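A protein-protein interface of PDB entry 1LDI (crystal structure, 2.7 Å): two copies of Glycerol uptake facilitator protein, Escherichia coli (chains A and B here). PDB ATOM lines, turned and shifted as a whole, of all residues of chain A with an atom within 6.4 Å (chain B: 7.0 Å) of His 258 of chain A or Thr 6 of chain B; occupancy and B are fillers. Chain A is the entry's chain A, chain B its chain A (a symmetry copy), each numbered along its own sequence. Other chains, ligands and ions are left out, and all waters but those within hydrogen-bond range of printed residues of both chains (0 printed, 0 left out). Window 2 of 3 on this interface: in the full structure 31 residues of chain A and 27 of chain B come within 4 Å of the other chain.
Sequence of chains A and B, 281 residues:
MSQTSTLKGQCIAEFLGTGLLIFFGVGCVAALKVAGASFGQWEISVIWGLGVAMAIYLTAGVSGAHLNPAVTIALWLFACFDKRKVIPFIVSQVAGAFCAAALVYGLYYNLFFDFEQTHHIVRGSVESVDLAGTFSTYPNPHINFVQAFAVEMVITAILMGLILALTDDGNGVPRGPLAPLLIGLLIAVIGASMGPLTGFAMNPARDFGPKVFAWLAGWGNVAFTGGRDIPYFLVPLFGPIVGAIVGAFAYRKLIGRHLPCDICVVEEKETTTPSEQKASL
The side-chain amide nitrogen of Gln 10 of chain B sits at hydrogen-bond distance from the backbone carbonyl oxygen of Val 62 of chain B.
Among the printed residues, merely in contact across the chains: Leu 254 of chain A with Ile 12 of chain B (3.8 Å), His 258 of chain A with Thr 6 of chain B (3.8 Å), His 258 of chain A with Gly 9 of chain B (3.8 Å), His 258 of chain A with Val 62 of chain B (3.96 Å) and Leu 259 of chain A with Val 62 of chain B (3.4 Å).
Of the printed residues of chain B, His 258 of chain A touches Thr 6, Gly 9 and Val 62.
Of chain A, only His 258 (3.8 Å) comes within 4 Å of Thr 6 of chain B.
Of the printed residues of chain B, Leu 259 of chain A touches Val 62.
Of the printed residues of chain A, Gly 9 of chain B touches His 258 (3.8 Å).
Printed residues of chain A within 4 Å of Ile 12 of chain B: Leu 254 (3.8 Å).
Of the printed residues of chain B, Leu 254 of chain A touches Ile 12 (3.8 Å).
Lys 8 of chain B touches none of the printed residues of chain A.
Lys 253 of chain A touches none of the printed residues of chain B.
The nearest printed residue of chain A that does not touch Thr 6 of chain B is Arg 257 of chain A (6.8 Å).
Along chain B the printed residues that touch a printed residue of chain A span positions 6 to 62.
Of the 8 printed residues of chain A, 3 touch a printed residue of chain B.
Printed residues of chain A that touch a printed residue of chain B: Leu 254, His 258 and Leu 259.
Hydrophobic or aromatic side chains of chain A that line the printed part of chain B: His 258 and Leu 259.
No position is printed for both chains.
Of the 5 pairs that touch across the chains among the printed residues, none has its exchanged pair printed and touching as well.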
ATOM      1  N   ARG A 252      22.795 -19.078 -17.439  1.00  0.00           N
ATOM      2  CA  ARG A 252      22.291 -20.410 -17.124  1.00  0.00           C
ATOM      3  C   ARG A 252      22.044 -21.251 -18.371  1.00  0.00           C
ATOM      4  O   ARG A 252      22.247 -22.466 -18.354  1.00  0.00           O
ATOM      5  CB  ARG A 252      21.001 -20.315 -16.294  1.00  0.00           C
ATOM      6  CG  ARG A 252      21.201 -19.698 -14.903  1.00  0.00           C
ATOM      7  CD  ARG A 252      20.600 -20.569 -13.793  1.00  0.00           C
ATOM      8  NE  ARG A 252      20.673 -19.934 -12.475  1.00  0.00           N
ATOM      9  CZ  ARG A 252      21.805 -19.596 -11.859  1.00  0.00           C
ATOM     10  NH1 ARG A 252      22.978 -19.832 -12.436  1.00  0.00           N
ATOM     11  NH2 ARG A 252      21.766 -19.015 -10.663  1.00  0.00           N
ATOM     12  N   LYS A 253      21.620 -20.603 -19.450  1.00  0.00           N
ATOM     13  CA  LYS A 253      21.345 -21.303 -20.697  1.00  0.00           C
ATOM     14  C   LYS A 253      22.574 -21.575 -21.558  1.00  0.00           C
ATOM     15  O   LYS A 253      22.934 -22.724 -21.796  1.00  0.00           O
ATOM     16  CB  LYS A 253      20.320 -20.520 -21.531  1.00  0.00           C
ATOM     17  CG  LYS A 253      18.915 -20.547 -20.966  1.00  0.00           C
ATOM     18  CD  LYS A 253      18.417 -21.981 -20.877  1.00  0.00           C
ATOM     19  CE  LYS A 253      17.364 -22.134 -19.797  1.00  0.00           C
ATOM     20  NZ  LYS A 253      17.369 -23.526 -19.255  1.00  0.00           N
ATOM     21  N   LEU A 254      23.226 -20.517 -22.013  1.00  0.00           N
ATOM     22  CA  LEU A 254      24.375 -20.646 -22.893  1.00  0.00           C
ATOM     23  C   LEU A 254      25.707 -21.076 -22.264  1.00  0.00           C
ATOM     24  O   LEU A 254      26.579 -21.590 -22.966  1.00  0.00           O
ATOM     25  CB  LEU A 254      24.559 -19.327 -23.645  1.00  0.00           C
ATOM     26  CG  LEU A 254      23.284 -18.737 -24.252  1.00  0.00           C
ATOM     27  CD1 LEU A 254      23.541 -17.309 -24.673  1.00  0.00           C
ATOM     28  CD2 LEU A 254      22.831 -19.573 -25.435  1.00  0.00           C
ATOM     29  N   ILE A 255      25.884 -20.869 -20.962  1.00  0.00           N
ATOM     30  CA  ILE A 255      27.146 -21.245 -20.325  1.00  0.00           C
ATOM     31  C   ILE A 255      26.994 -22.293 -19.227  1.00  0.00           C
ATOM     32  O   ILE A 255      27.629 -23.344 -19.278  1.00  0.00           O
ATOM     33  CB  ILE A 255      27.880 -20.002 -19.738  1.00  0.00           C
ATOM     34  CG1 ILE A 255      28.153 -18.986 -20.847  1.00  0.00           C
ATOM     35  CG2 ILE A 255      29.204 -20.412 -19.095  1.00  0.00           C
ATOM     36  CD1 ILE A 255      29.009 -19.510 -21.972  1.00  0.00           C
ATOM     37  N   GLY A 256      26.160 -22.008 -18.235  1.00  0.00           N
ATOM     38  CA  GLY A 256      25.965 -22.948 -17.147  1.00  0.00           C
ATOM     39  C   GLY A 256      25.559 -24.326 -17.628  1.00  0.00           C
ATOM     40  O   GLY A 256      26.098 -25.333 -17.174  1.00  0.00           O
ATOM     41  N   ARG A 257      24.609 -24.369 -18.557  1.00  0.00           N
ATOM     42  CA  ARG A 257      24.110 -25.629 -19.104  1.00  0.00           C
ATOM     43  C   ARG A 257      25.218 -26.503 -19.684  1.00  0.00           C
ATOM     44  O   ARG A 257      25.064 -27.726 -19.776  1.00  0.00           O
ATOM     45  CB  ARG A 257      23.056 -25.353 -20.177  1.00  0.00           C
ATOM     46  N   HIS A 258      26.332 -25.878 -20.067  1.00  0.00           N
ATOM     47  CA  HIS A 258      27.453 -26.608 -20.650  1.00  0.00           C
ATOM     48  C   HIS A 258      28.688 -26.676 -19.762  1.00  0.00           C
ATOM     49  O   HIS A 258      29.818 -26.627 -20.246  1.00  0.00           O
ATOM     50  CB  HIS A 258      27.811 -26.001 -22.005  1.00  0.00           C
ATOM     51  CG  HIS A 258      26.665 -25.988 -22.964  1.00  0.00           C
ATOM     52  ND1 HIS A 258      25.652 -25.055 -22.900  1.00  0.00           N
ATOM     53  CD2 HIS A 258      26.334 -26.833 -23.969  1.00  0.00           C
ATOM     54  CE1 HIS A 258      24.746 -25.326 -23.824  1.00  0.00           C
ATOM     55  NE2 HIS A 258      25.136 -26.400 -24.486  1.00  0.00           N
ATOM     56  N   LEU A 259      28.459 -26.810 -18.460  1.00  0.00           N
ATOM     57  CA  LEU A 259      29.537 -26.897 -17.486  1.00  0.00           C
ATOM     58  C   LEU A 259      29.507 -28.249 -16.771  1.00  0.00           C
ATOM     59  O   LEU A 259      30.575 -28.900 -16.656  1.00  0.00           O
ATOM     60  CB  LEU A 259      29.411 -25.765 -16.464  1.00  0.00           C
ATOM     61  CG  LEU A 259      29.754 -24.354 -16.946  1.00  0.00           C
ATOM     62  CD1 LEU A 259      29.376 -23.344 -15.879  1.00  0.00           C
ATOM     63  CD2 LEU A 259      31.235 -24.273 -17.266  1.00  0.00           C
ATOM     64  N   THR B   6      31.576 -30.522 -25.056  1.00  0.00           N
ATOM     65  CA  THR B   6      30.797 -30.578 -26.329  1.00  0.00           C
ATOM     66  C   THR B   6      31.117 -29.388 -27.231  1.00  0.00           C
ATOM     67  O   THR B   6      30.907 -28.233 -26.858  1.00  0.00           O
ATOM     68  CB  THR B   6      29.267 -30.611 -26.064  1.00  0.00           C
ATOM     69  OG1 THR B   6      28.564 -30.452 -27.303  1.00  0.00           O
ATOM     70  CG2 THR B   6      28.854 -29.498 -25.105  1.00  0.00           C
ATOM     71  N   LEU B   7      31.619 -29.696 -28.421  1.00  0.00           N
ATOM     72  CA  LEU B   7      32.010 -28.696 -29.406  1.00  0.00           C
ATOM     73  C   LEU B   7      31.029 -27.551 -29.660  1.00  0.00           C
ATOM     74  O   LEU B   7      31.452 -26.440 -29.980  1.00  0.00           O
ATOM     75  CB  LEU B   7      32.336 -29.382 -30.736  1.00  0.00           C
ATOM     76  CG  LEU B   7      32.863 -28.442 -31.824  1.00  0.00           C
ATOM     77  CD1 LEU B   7      34.085 -27.701 -31.290  1.00  0.00           C
ATOM     78  CD2 LEU B   7      33.217 -29.231 -33.071  1.00  0.00           C
ATOM     79  N   LYS B   8      29.731 -27.809 -29.538  1.00  0.00           N
ATOM     80  CA  LYS B   8      28.751 -26.751 -29.767  1.00  0.00           C
ATOM     81  C   LYS B   8      28.798 -25.750 -28.617  1.00  0.00           C
ATOM     82  O   LYS B   8      28.661 -24.543 -28.818  1.00  0.00           O
ATOM     83  CB  LYS B   8      27.337 -27.331 -29.885  1.00  0.00           C
ATOM     84  CG  LYS B   8      26.286 -26.300 -30.289  1.00  0.00           C
ATOM     85  CD  LYS B   8      24.890 -26.895 -30.346  1.00  0.00           C
ATOM     86  CE  LYS B   8      23.876 -25.846 -30.791  1.00  0.00           C
ATOM     87  NZ  LYS B   8      22.472 -26.365 -30.842  1.00  0.00           N
ATOM     88  N   GLY B   9      28.995 -26.268 -27.409  1.00  0.00           N
ATOM     89  CA  GLY B   9      29.058 -25.418 -26.235  1.00  0.00           C
ATOM     90  C   GLY B   9      30.359 -24.646 -26.153  1.00  0.00           C
ATOM     91  O   GLY B   9      30.433 -23.591 -25.510  1.00  0.00           O
ATOM     92  N   GLN B  10      31.392 -25.180 -26.795  1.00  0.00           N
ATOM     93  CA  GLN B  10      32.688 -24.526 -26.811  1.00  0.00           C
ATOM     94  C   GLN B  10      32.680 -23.398 -27.837  1.00  0.00           C
ATOM     95  O   GLN B  10      33.290 -22.354 -27.635  1.00  0.00           O
ATOM     96  CB  GLN B  10      33.777 -25.521 -27.174  1.00  0.00           C
ATOM     97  CG  GLN B  10      33.855 -26.701 -26.257  1.00  0.00           C
ATOM     98  CD  GLN B  10      35.201 -27.343 -26.342  1.00  0.00           C
ATOM     99  OE1 GLN B  10      35.651 -27.716 -27.422  1.00  0.00           O
ATOM    100  NE2 GLN B  10      35.871 -27.465 -25.205  1.00  0.00           N
ATOM    101  N   CYS B  11      31.991 -23.623 -28.946  1.00  0.00           N
ATOM    102  CA  CYS B  11      31.892 -22.620 -29.991  1.00  0.00           C
ATOM    103  C   CYS B  11      31.062 -21.454 -29.470  1.00  0.00           C
ATOM    104  O   CYS B  11      31.329 -20.293 -29.784  1.00  0.00           O
ATOM    105  CB  CYS B  11      31.257 -23.229 -31.247  1.00  0.00           C
ATOM    106  SG  CYS B  11      32.334 -24.432 -32.055  1.00  0.00           S
ATOM    107  N   ILE B  12      30.056 -21.765 -28.665  1.00  0.00           N
ATOM    108  CA  ILE B  12      29.220 -20.722 -28.100  1.00  0.00           C
ATOM    109  C   ILE B  12      30.074 -19.867 -27.164  1.00  0.00           C
ATOM    110  O   ILE B  12      30.008 -18.635 -27.195  1.00  0.00           O
ATOM    111  CB  ILE B  12      28.011 -21.328 -27.338  1.00  0.00           C
ATOM    112  CG1 ILE B  12      27.028 -21.917 -28.349  1.00  0.00           C
ATOM    113  CG2 ILE B  12      27.317 -20.266 -26.490  1.00  0.00           C
ATOM    114  CD1 ILE B  12      25.734 -22.371 -27.745  1.00  0.00           C
ATOM    115  N   GLY B  61      36.743 -22.080 -18.646  1.00  0.00           N
ATOM    116  CA  GLY B  61      36.219 -23.342 -18.147  1.00  0.00           C
ATOM    117  C   GLY B  61      35.524 -24.220 -19.167  1.00  0.00           C
ATOM    118  O   GLY B  61      35.425 -25.433 -18.995  1.00  0.00           O
ATOM    119  N   VAL B  62      35.044 -23.610 -20.241  1.00  0.00           N
ATOM    120  CA  VAL B  62      34.348 -24.352 -21.277  1.00  0.00           C
ATOM    121  C   VAL B  62      35.197 -24.575 -22.531  1.00  0.00           C
ATOM    122  O   VAL B  62      35.650 -25.690 -22.793  1.00  0.00           O
ATOM    123  CB  VAL B  62      33.047 -23.632 -21.666  1.00  0.00           C
ATOM    124  CG1 VAL B  62      32.312 -24.419 -22.723  1.00  0.00           C
ATOM    125  CG2 VAL B  62      32.176 -23.451 -20.443  1.00  0.00           C
ATOM    126  N   LYS B  85      38.616 -29.285 -34.108  1.00  0.00           N
ATOM    127  CA  LYS B  85      38.078 -28.115 -33.410  1.00  0.00           C
ATOM    128  C   LYS B  85      38.597 -26.760 -33.908  1.00  0.00           C
ATOM    129  O   LYS B  85      38.055 -25.714 -33.562  1.00  0.00           O
ATOM    130  CB  LYS B  85      38.372 -28.242 -31.917  1.00  0.00           C
ATOM    131  CG  LYS B  85      37.536 -29.275 -31.196  1.00  0.00           C
ATOM    132  CD  LYS B  85      37.864 -29.296 -29.705  1.00  0.00           C
ATOM    133  CE  LYS B  85      36.860 -30.121 -28.914  1.00  0.00           C
ATOM    134  NZ  LYS B  85      36.798 -31.529 -29.398  1.00  0.00           N
